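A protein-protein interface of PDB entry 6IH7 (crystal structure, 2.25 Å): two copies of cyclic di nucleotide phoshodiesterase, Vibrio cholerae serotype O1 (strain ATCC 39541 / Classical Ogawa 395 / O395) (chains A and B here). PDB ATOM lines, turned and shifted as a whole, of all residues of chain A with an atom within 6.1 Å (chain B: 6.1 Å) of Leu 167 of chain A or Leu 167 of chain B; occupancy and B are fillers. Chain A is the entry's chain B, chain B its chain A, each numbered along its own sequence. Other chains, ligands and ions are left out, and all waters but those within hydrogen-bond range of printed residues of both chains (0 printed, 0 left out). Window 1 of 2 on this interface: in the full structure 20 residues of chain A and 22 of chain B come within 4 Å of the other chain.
The backbone carbonyl oxygen of Ile 197 of chain A sits at hydrogen-bond distance from the side-chain sulfur of Cys 201 of chain A (3.3 Å). OG of Ser 165 of chain A is in hydrogen-bond range of N of Phe 160 of chain A (3.4 Å). OD1 of Asn 168 of chain A lies close to O of Gly 166 of chain A (3.3 Å). The backbone carbonyl oxygen (O) of Ile 197 of chain B is in hydrogen-bond range of the side-chain sulfur (SG) of Cys 201 of chain B, at 3.3 Å. N of Gly 166 of chain B sits close to OD1 of Asn 168 of chain B.
Leu 167 of chain B touches Phe 160 of chain A. CD1 of Leu 167 of chain A touches CD1 of Leu 167 of chain B (3.9 Å). Ile 197 of chain B touches Leu 167 of chain A (CD1 to O, 3.9 Å). Cys 201 of chain B touches Leu 167 of chain A (SG to CD1, 3.9 Å). Asn 168 of chain A touches Gly 161 of chain B. CD2 of Leu 184 of chain A touches CB of Ala 171 of chain B, 3.7 Å away. Ala 171 of chain B touches Ile 197 of chain A. Ile 197 of chain A touches Leu 204 of chain B (N to CD1, 3.6 Å). CD1 of Leu 167 of chain B touches SG of Cys 201 of chain A (3.8 Å). Leu 204 of chain A touches Ile 197 of chain B.
Printed residues of chain B within 4 Å of Leu 167 of chain A: Phe 160, Leu 167, Ile 197 and Cys 201. Of the printed residues of chain B, Ile 197 of chain A touches Leu 167 (3.9 Å), Ala 171 (3.6 Å) and Leu 204 (3.6 Å). Of the printed residues of chain B, Leu 204 of chain A touches Ile 197 (3.8 Å). Ser 165 of chain B touches none of the printed residues of chain A. Of the printed residues of chain A, Leu 167 of chain B touches Phe 160, Leu 167, Ile 197 and Cys 201.
Hydrophobic or aromatic side chains of chain A that line the printed part of chain B: Phe 160, Leu 167, Ala 171, Leu 184, Ile 197 and Leu 204. Along chain A the printed residues that touch a printed residue of chain B span positions 160 to 204. Among the printed residues, 16 pairs touch across the chains. Among the printed residues, no Asp or Glu carboxylate lies within 4 Å of a Lys or Arg side-chain nitrogen of the other chain.
Leu 167 of chain B touches its own counterpart, Leu 167 of chain A. Leu 167 of chain A touches Ile 197 of chain B, and with the chains exchanged Ile 197 of chain A touches Leu 167 of chain B. Ala 171 of chain A touches Leu 184 of chain B, and with the chains exchanged Leu 184 of chain A touches Ala 171 of chain B. Ile 197 of chain A touches Leu 204 of chain B, and with the chains exchanged Leu 204 of chain A touches Ile 197 of chain B. Of the 16 pairs that touch across the chains among the printed residues, 15 have their exchanged pair printed and touching as well.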
ATOM      1  N   PHE A 160      29.121 -21.784 -19.641  1.00  0.00           N
ATOM      2  CA  PHE A 160      28.454 -22.625 -20.625  1.00  0.00           C
ATOM      3  C   PHE A 160      28.500 -21.952 -21.996  1.00  0.00           C
ATOM      4  O   PHE A 160      28.159 -20.776 -22.136  1.00  0.00           O
ATOM      5  CB  PHE A 160      27.018 -22.881 -20.194  1.00  0.00           C
ATOM      6  CG  PHE A 160      26.245 -23.748 -21.141  1.00  0.00           C
ATOM      7  CD1 PHE A 160      26.224 -25.119 -20.979  1.00  0.00           C
ATOM      8  CD2 PHE A 160      25.524 -23.185 -22.179  1.00  0.00           C
ATOM      9  CE1 PHE A 160      25.528 -25.916 -21.858  1.00  0.00           C
ATOM     10  CE2 PHE A 160      24.820 -23.974 -23.049  1.00  0.00           C
ATOM     11  CZ  PHE A 160      24.815 -25.357 -22.878  1.00  0.00           C
ATOM     12  N   GLY A 161      28.940 -22.686 -23.011  1.00  0.00           N
ATOM     13  CA  GLY A 161      29.110 -22.081 -24.314  1.00  0.00           C
ATOM     14  C   GLY A 161      30.505 -21.569 -24.584  1.00  0.00           C
ATOM     15  O   GLY A 161      30.700 -20.801 -25.531  1.00  0.00           O
ATOM     16  N   TYR A 164      35.535 -25.765 -22.292  1.00  0.00           N
ATOM     17  CA  TYR A 164      35.065 -27.131 -22.131  1.00  0.00           C
ATOM     18  C   TYR A 164      33.653 -27.200 -21.593  1.00  0.00           C
ATOM     19  O   TYR A 164      32.986 -28.232 -21.755  1.00  0.00           O
ATOM     20  CB  TYR A 164      35.968 -27.912 -21.180  1.00  0.00           C
ATOM     21  CG  TYR A 164      35.906 -29.377 -21.465  1.00  0.00           C
ATOM     22  CD1 TYR A 164      35.022 -30.212 -20.794  1.00  0.00           C
ATOM     23  CD2 TYR A 164      36.697 -29.918 -22.446  1.00  0.00           C
ATOM     24  CE1 TYR A 164      34.970 -31.554 -21.073  1.00  0.00           C
ATOM     25  CE2 TYR A 164      36.644 -31.233 -22.733  1.00  0.00           C
ATOM     26  CZ  TYR A 164      35.783 -32.063 -22.059  1.00  0.00           C
ATOM     27  OH  TYR A 164      35.752 -33.404 -22.378  1.00  0.00           O
ATOM     28  N   SER A 165      33.201 -26.136 -20.950  1.00  0.00           N
ATOM     29  CA  SER A 165      31.879 -26.106 -20.346  1.00  0.00           C
ATOM     30  C   SER A 165      30.847 -26.130 -21.461  1.00  0.00           C
ATOM     31  O   SER A 165      30.541 -25.103 -22.073  1.00  0.00           O
ATOM     32  CB  SER A 165      31.744 -24.879 -19.460  1.00  0.00           C
ATOM     33  OG  SER A 165      30.453 -24.817 -18.904  1.00  0.00           O
ATOM     34  N   GLY A 166      30.330 -27.321 -21.741  1.00  0.00           N
ATOM     35  CA  GLY A 166      29.438 -27.519 -22.858  1.00  0.00           C
ATOM     36  C   GLY A 166      28.281 -28.444 -22.563  1.00  0.00           C
ATOM     37  O   GLY A 166      27.968 -28.749 -21.403  1.00  0.00           O
ATOM     38  N   LEU A 167      27.611 -28.852 -23.636  1.00  0.00           N
ATOM     39  CA  LEU A 167      26.495 -29.779 -23.536  1.00  0.00           C
ATOM     40  C   LEU A 167      26.927 -31.101 -22.927  1.00  0.00           C
ATOM     41  O   LEU A 167      26.112 -31.791 -22.307  1.00  0.00           O
ATOM     42  CB  LEU A 167      25.888 -29.975 -24.937  1.00  0.00           C
ATOM     43  CG  LEU A 167      25.329 -28.617 -25.402  1.00  0.00           C
ATOM     44  CD1 LEU A 167      25.283 -28.490 -26.922  1.00  0.00           C
ATOM     45  CD2 LEU A 167      23.930 -28.412 -24.799  1.00  0.00           C
ATOM     46  N   ASN A 168      28.199 -31.478 -23.115  1.00  0.00           N
ATOM     47  CA  ASN A 168      28.719 -32.720 -22.551  1.00  0.00           C
ATOM     48  C   ASN A 168      28.553 -32.762 -21.044  1.00  0.00           C
ATOM     49  O   ASN A 168      28.399 -33.841 -20.473  1.00  0.00           O
ATOM     50  CB  ASN A 168      30.192 -32.869 -22.901  1.00  0.00           C
ATOM     51  CG  ASN A 168      30.976 -31.601 -22.614  1.00  0.00           C
ATOM     52  OD1 ASN A 168      30.441 -30.496 -22.697  1.00  0.00           O
ATOM     53  ND2 ASN A 168      32.235 -31.754 -22.244  1.00  0.00           N
ATOM     54  N   LEU A 169      28.591 -31.599 -20.385  1.00  0.00           N
ATOM     55  CA  LEU A 169      28.339 -31.545 -18.948  1.00  0.00           C
ATOM     56  C   LEU A 169      26.863 -31.760 -18.651  1.00  0.00           C
ATOM     57  O   LEU A 169      26.506 -32.652 -17.871  1.00  0.00           O
ATOM     58  CB  LEU A 169      28.832 -30.210 -18.385  1.00  0.00           C
ATOM     59  CG  LEU A 169      30.337 -30.077 -18.613  1.00  0.00           C
ATOM     60  CD1 LEU A 169      30.918 -28.799 -18.057  1.00  0.00           C
ATOM     61  CD2 LEU A 169      31.035 -31.283 -18.011  1.00  0.00           C
ATOM     62  N   LEU A 170      25.985 -30.977 -19.294  1.00  0.00           N
ATOM     63  CA  LEU A 170      24.540 -31.148 -19.103  1.00  0.00           C
ATOM     64  C   LEU A 170      24.076 -32.580 -19.362  1.00  0.00           C
ATOM     65  O   LEU A 170      23.085 -33.028 -18.777  1.00  0.00           O
ATOM     66  CB  LEU A 170      23.774 -30.193 -20.014  1.00  0.00           C
ATOM     67  CG  LEU A 170      23.811 -28.754 -19.534  1.00  0.00           C
ATOM     68  CD1 LEU A 170      23.003 -27.859 -20.467  1.00  0.00           C
ATOM     69  CD2 LEU A 170      23.257 -28.709 -18.109  1.00  0.00           C
ATOM     70  N   ALA A 171      24.744 -33.302 -20.261  1.00  0.00           N
ATOM     71  CA  ALA A 171      24.255 -34.622 -20.633  1.00  0.00           C
ATOM     72  C   ALA A 171      24.303 -35.586 -19.449  1.00  0.00           C
ATOM     73  O   ALA A 171      23.412 -36.431 -19.280  1.00  0.00           O
ATOM     74  CB  ALA A 171      25.074 -35.166 -21.800  1.00  0.00           C
ATOM     75  N   ASP A 172      25.338 -35.476 -18.620  1.00  0.00           N
ATOM     76  CA  ASP A 172      25.557 -36.434 -17.555  1.00  0.00           C
ATOM     77  C   ASP A 172      25.081 -35.958 -16.182  1.00  0.00           C
ATOM     78  O   ASP A 172      24.751 -36.808 -15.347  1.00  0.00           O
ATOM     79  CB  ASP A 172      27.043 -36.823 -17.529  1.00  0.00           C
ATOM     80  CG  ASP A 172      27.435 -37.663 -18.748  1.00  0.00           C
ATOM     81  OD1 ASP A 172      26.744 -38.658 -19.021  1.00  0.00           O
ATOM     82  OD2 ASP A 172      28.373 -37.292 -19.479  1.00  0.00           O
ATOM     83  N   LEU A 184      28.494 -15.764 -25.688  1.00  0.00           N
ATOM     84  CA  LEU A 184      27.182 -16.003 -26.283  1.00  0.00           C
ATOM     85  C   LEU A 184      26.205 -14.860 -26.044  1.00  0.00           C
ATOM     86  O   LEU A 184      25.183 -14.772 -26.737  1.00  0.00           O
ATOM     87  CB  LEU A 184      26.569 -17.294 -25.729  1.00  0.00           C
ATOM     88  CG  LEU A 184      27.244 -18.642 -26.017  1.00  0.00           C
ATOM     89  CD1 LEU A 184      26.403 -19.816 -25.595  1.00  0.00           C
ATOM     90  CD2 LEU A 184      27.554 -18.728 -27.521  1.00  0.00           C
ATOM     91  N   ILE A 197      20.820 -19.577 -30.827  1.00  0.00           N
ATOM     92  CA  ILE A 197      21.507 -20.391 -29.820  1.00  0.00           C
ATOM     93  C   ILE A 197      20.836 -20.219 -28.461  1.00  0.00           C
ATOM     94  O   ILE A 197      20.490 -21.194 -27.777  1.00  0.00           O
ATOM     95  CB  ILE A 197      22.998 -20.022 -29.749  1.00  0.00           C
ATOM     96  CG1 ILE A 197      23.729 -20.439 -31.024  1.00  0.00           C
ATOM     97  CG2 ILE A 197      23.652 -20.632 -28.513  1.00  0.00           C
ATOM     98  CD1 ILE A 197      25.240 -20.292 -30.927  1.00  0.00           C
ATOM     99  N   CYS A 201      18.686 -22.929 -26.340  1.00  0.00           N
ATOM    100  CA  CYS A 201      19.258 -23.347 -25.056  1.00  0.00           C
ATOM    101  C   CYS A 201      18.296 -23.105 -23.884  1.00  0.00           C
ATOM    102  O   CYS A 201      18.160 -23.960 -22.997  1.00  0.00           O
ATOM    103  CB  CYS A 201      20.591 -22.644 -24.815  1.00  0.00           C
ATOM    104  SG  CYS A 201      21.937 -23.395 -25.794  1.00  0.00           S
ATOM    105  N   LEU A 204      15.980 -25.803 -23.754  1.00  0.00           N
ATOM    106  CA  LEU A 204      16.705 -26.911 -23.147  1.00  0.00           C
ATOM    107  C   LEU A 204      16.757 -26.762 -21.619  1.00  0.00           C
ATOM    108  O   LEU A 204      16.433 -27.700 -20.875  1.00  0.00           O
ATOM    109  CB  LEU A 204      18.109 -26.999 -23.739  1.00  0.00           C
ATOM    110  CG  LEU A 204      19.019 -28.031 -23.081  1.00  0.00           C
ATOM    111  CD1 LEU A 204      18.379 -29.401 -23.109  1.00  0.00           C
ATOM    112  CD2 LEU A 204      20.326 -28.084 -23.797  1.00  0.00           C
ATOM    113  N   PHE B 160      30.562 -32.394 -32.034  1.00  0.00           N
ATOM    114  CA  PHE B 160      29.769 -31.356 -31.393  1.00  0.00           C
ATOM    115  C   PHE B 160      29.131 -31.903 -30.120  1.00  0.00           C
ATOM    116  O   PHE B 160      28.572 -33.004 -30.111  1.00  0.00           O
ATOM    117  CB  PHE B 160      28.684 -30.844 -32.331  1.00  0.00           C
ATOM    118  CG  PHE B 160      27.754 -29.825 -31.692  1.00  0.00           C
ATOM    119  CD1 PHE B 160      28.073 -28.476 -31.679  1.00  0.00           C
ATOM    120  CD2 PHE B 160      26.572 -30.228 -31.072  1.00  0.00           C
ATOM    121  CE1 PHE B 160      27.223 -27.563 -31.073  1.00  0.00           C
ATOM    122  CE2 PHE B 160      25.720 -29.300 -30.465  1.00  0.00           C
ATOM    123  CZ  PHE B 160      26.050 -27.973 -30.477  1.00  0.00           C
ATOM    124  N   GLY B 161      29.200 -31.131 -29.041  1.00  0.00           N
ATOM    125  CA  GLY B 161      28.628 -31.609 -27.804  1.00  0.00           C
ATOM    126  C   GLY B 161      29.578 -32.447 -27.001  1.00  0.00           C
ATOM    127  O   GLY B 161      29.160 -33.144 -26.069  1.00  0.00           O
ATOM    128  N   SER B 162      30.855 -32.411 -27.342  1.00  0.00           N
ATOM    129  CA  SER B 162      31.867 -33.033 -26.519  1.00  0.00           C
ATOM    130  C   SER B 162      33.079 -32.133 -26.483  1.00  0.00           C
ATOM    131  O   SER B 162      33.257 -31.263 -27.338  1.00  0.00           O
ATOM    132  CB  SER B 162      32.312 -34.376 -27.064  1.00  0.00           C
ATOM    133  OG  SER B 162      33.496 -34.157 -27.801  1.00  0.00           O
ATOM    134  N   SER B 165      34.626 -28.690 -28.383  1.00  0.00           N
ATOM    135  CA  SER B 165      33.894 -28.454 -29.633  1.00  0.00           C
ATOM    136  C   SER B 165      32.404 -28.355 -29.316  1.00  0.00           C
ATOM    137  O   SER B 165      31.734 -29.368 -29.093  1.00  0.00           O
ATOM    138  CB  SER B 165      34.196 -29.568 -30.636  1.00  0.00           C
ATOM    139  OG  SER B 165      33.313 -29.578 -31.752  1.00  0.00           O
ATOM    140  N   GLY B 166      31.889 -27.127 -29.287  1.00  0.00           N
ATOM    141  CA  GLY B 166      30.494 -26.931 -28.977  1.00  0.00           C
ATOM    142  C   GLY B 166      29.869 -25.665 -29.521  1.00  0.00           C
ATOM    143  O   GLY B 166      30.123 -25.254 -30.660  1.00  0.00           O
ATOM    144  N   LEU B 167      29.032 -25.049 -28.683  1.00  0.00           N
ATOM    145  CA  LEU B 167      28.228 -23.913 -29.100  1.00  0.00           C
ATOM    146  C   LEU B 167      29.088 -22.699 -29.394  1.00  0.00           C
ATOM    147  O   LEU B 167      28.733 -21.890 -30.258  1.00  0.00           O
ATOM    148  CB  LEU B 167      27.186 -23.605 -28.019  1.00  0.00           C
ATOM    149  CG  LEU B 167      26.170 -24.740 -27.831  1.00  0.00           C
ATOM    150  CD1 LEU B 167      25.405 -24.667 -26.475  1.00  0.00           C
ATOM    151  CD2 LEU B 167      25.191 -24.774 -29.015  1.00  0.00           C
ATOM    152  N   ASN B 168      30.210 -22.550 -28.683  1.00  0.00           N
ATOM    153  CA  ASN B 168      31.096 -21.426 -28.944  1.00  0.00           C
ATOM    154  C   ASN B 168      31.515 -21.389 -30.397  1.00  0.00           C
ATOM    155  O   ASN B 168      31.729 -20.304 -30.942  1.00  0.00           O
ATOM    156  CB  ASN B 168      32.329 -21.473 -28.037  1.00  0.00           C
ATOM    157  CG  ASN B 168      33.075 -22.786 -28.118  1.00  0.00           C
ATOM    158  OD1 ASN B 168      32.514 -23.828 -28.470  1.00  0.00           O
ATOM    159  ND2 ASN B 168      34.361 -22.743 -27.783  1.00  0.00           N
ATOM    160  N   LEU B 169      31.609 -22.556 -31.044  1.00  0.00           N
ATOM    161  CA  LEU B 169      31.963 -22.603 -32.459  1.00  0.00           C
ATOM    162  C   LEU B 169      30.806 -22.138 -33.333  1.00  0.00           C
ATOM    163  O   LEU B 169      30.986 -21.288 -34.213  1.00  0.00           O
ATOM    164  CB  LEU B 169      32.395 -24.020 -32.837  1.00  0.00           C
ATOM    165  CG  LEU B 169      33.728 -24.395 -32.204  1.00  0.00           C
ATOM    166  CD1 LEU B 169      34.170 -25.787 -32.569  1.00  0.00           C
ATOM    167  CD2 LEU B 169      34.739 -23.375 -32.667  1.00  0.00           C
ATOM    168  N   LEU B 170      29.602 -22.678 -33.094  1.00  0.00           N
ATOM    169  CA  LEU B 170      28.444 -22.320 -33.910  1.00  0.00           C
ATOM    170  C   LEU B 170      28.131 -20.828 -33.857  1.00  0.00           C
ATOM    171  O   LEU B 170      27.519 -20.292 -34.790  1.00  0.00           O
ATOM    172  CB  LEU B 170      27.217 -23.094 -33.450  1.00  0.00           C
ATOM    173  CG  LEU B 170      27.063 -24.514 -33.941  1.00  0.00           C
ATOM    174  CD1 LEU B 170      25.700 -25.029 -33.507  1.00  0.00           C
ATOM    175  CD2 LEU B 170      27.218 -24.519 -35.462  1.00  0.00           C
ATOM    176  N   ALA B 171      28.499 -20.155 -32.757  1.00  0.00           N
ATOM    177  CA  ALA B 171      28.109 -18.765 -32.568  1.00  0.00           C
ATOM    178  C   ALA B 171      28.827 -17.843 -33.546  1.00  0.00           C
ATOM    179  O   ALA B 171      28.251 -16.843 -33.984  1.00  0.00           O
ATOM    180  CB  ALA B 171      28.378 -18.334 -31.113  1.00  0.00           C
ATOM    181  N   ASP B 172      30.064 -18.166 -33.911  1.00  0.00           N
ATOM    182  CA  ASP B 172      30.843 -17.313 -34.798  1.00  0.00           C
ATOM    183  C   ASP B 172      30.998 -17.819 -36.234  1.00  0.00           C
ATOM    184  O   ASP B 172      31.340 -17.020 -37.111  1.00  0.00           O
ATOM    185  CB  ASP B 172      32.224 -17.071 -34.181  1.00  0.00           C
ATOM    186  CG  ASP B 172      32.149 -16.113 -33.011  1.00  0.00           C
ATOM    187  OD1 ASP B 172      31.482 -15.062 -33.171  1.00  0.00           O
ATOM    188  OD2 ASP B 172      32.708 -16.418 -31.934  1.00  0.00           O
ATOM    189  N   LEU B 184      26.776 -37.871 -26.955  1.00  0.00           N
ATOM    190  CA  LEU B 184      25.413 -37.364 -26.880  1.00  0.00           C
ATOM    191  C   LEU B 184      24.418 -38.339 -27.465  1.00  0.00           C
ATOM    192  O   LEU B 184      23.230 -38.250 -27.152  1.00  0.00           O
ATOM    193  CB  LEU B 184      25.296 -36.019 -27.611  1.00  0.00           C
ATOM    194  CG  LEU B 184      26.005 -34.838 -26.977  1.00  0.00           C
ATOM    195  CD1 LEU B 184      25.612 -33.538 -27.655  1.00  0.00           C
ATOM    196  CD2 LEU B 184      25.640 -34.765 -25.505  1.00  0.00           C
ATOM    197  N   ILE B 197      18.470 -32.640 -25.025  1.00  0.00           N
ATOM    198  CA  ILE B 197      19.593 -31.959 -25.664  1.00  0.00           C
ATOM    199  C   ILE B 197      19.468 -32.066 -27.185  1.00  0.00           C
ATOM    200  O   ILE B 197      19.550 -31.066 -27.903  1.00  0.00           O
ATOM    201  CB  ILE B 197      20.929 -32.542 -25.166  1.00  0.00           C
ATOM    202  CG1 ILE B 197      21.094 -32.297 -23.666  1.00  0.00           C
ATOM    203  CG2 ILE B 197      22.107 -32.026 -26.058  1.00  0.00           C
ATOM    204  CD1 ILE B 197      22.404 -32.756 -23.123  1.00  0.00           C
ATOM    205  N   CYS B 201      18.920 -29.135 -29.856  1.00  0.00           N
ATOM    206  CA  CYS B 201      19.991 -28.894 -30.827  1.00  0.00           C
ATOM    207  C   CYS B 201      19.483 -29.036 -32.262  1.00  0.00           C
ATOM    208  O   CYS B 201      19.824 -28.226 -33.141  1.00  0.00           O
ATOM    209  CB  CYS B 201      21.172 -29.836 -30.567  1.00  0.00           C
ATOM    210  SG  CYS B 201      22.106 -29.388 -29.040  1.00  0.00           S
ATOM    211  N   LEU B 204      17.820 -25.914 -33.216  1.00  0.00           N
ATOM    212  CA  LEU B 204      18.857 -24.913 -33.441  1.00  0.00           C
ATOM    213  C   LEU B 204      19.560 -25.125 -34.791  1.00  0.00           C
ATOM    214  O   LEU B 204      19.789 -24.159 -35.534  1.00  0.00           O
ATOM    215  CB  LEU B 204      19.865 -24.958 -32.300  1.00  0.00           C
ATOM    216  CG  LEU B 204      21.180 -24.234 -32.573  1.00  0.00           C
ATOM    217  CD1 LEU B 204      20.989 -22.741 -32.605  1.00  0.00           C
ATOM    218  CD2 LEU B 204      22.210 -24.640 -31.538  1.00  0.00           C
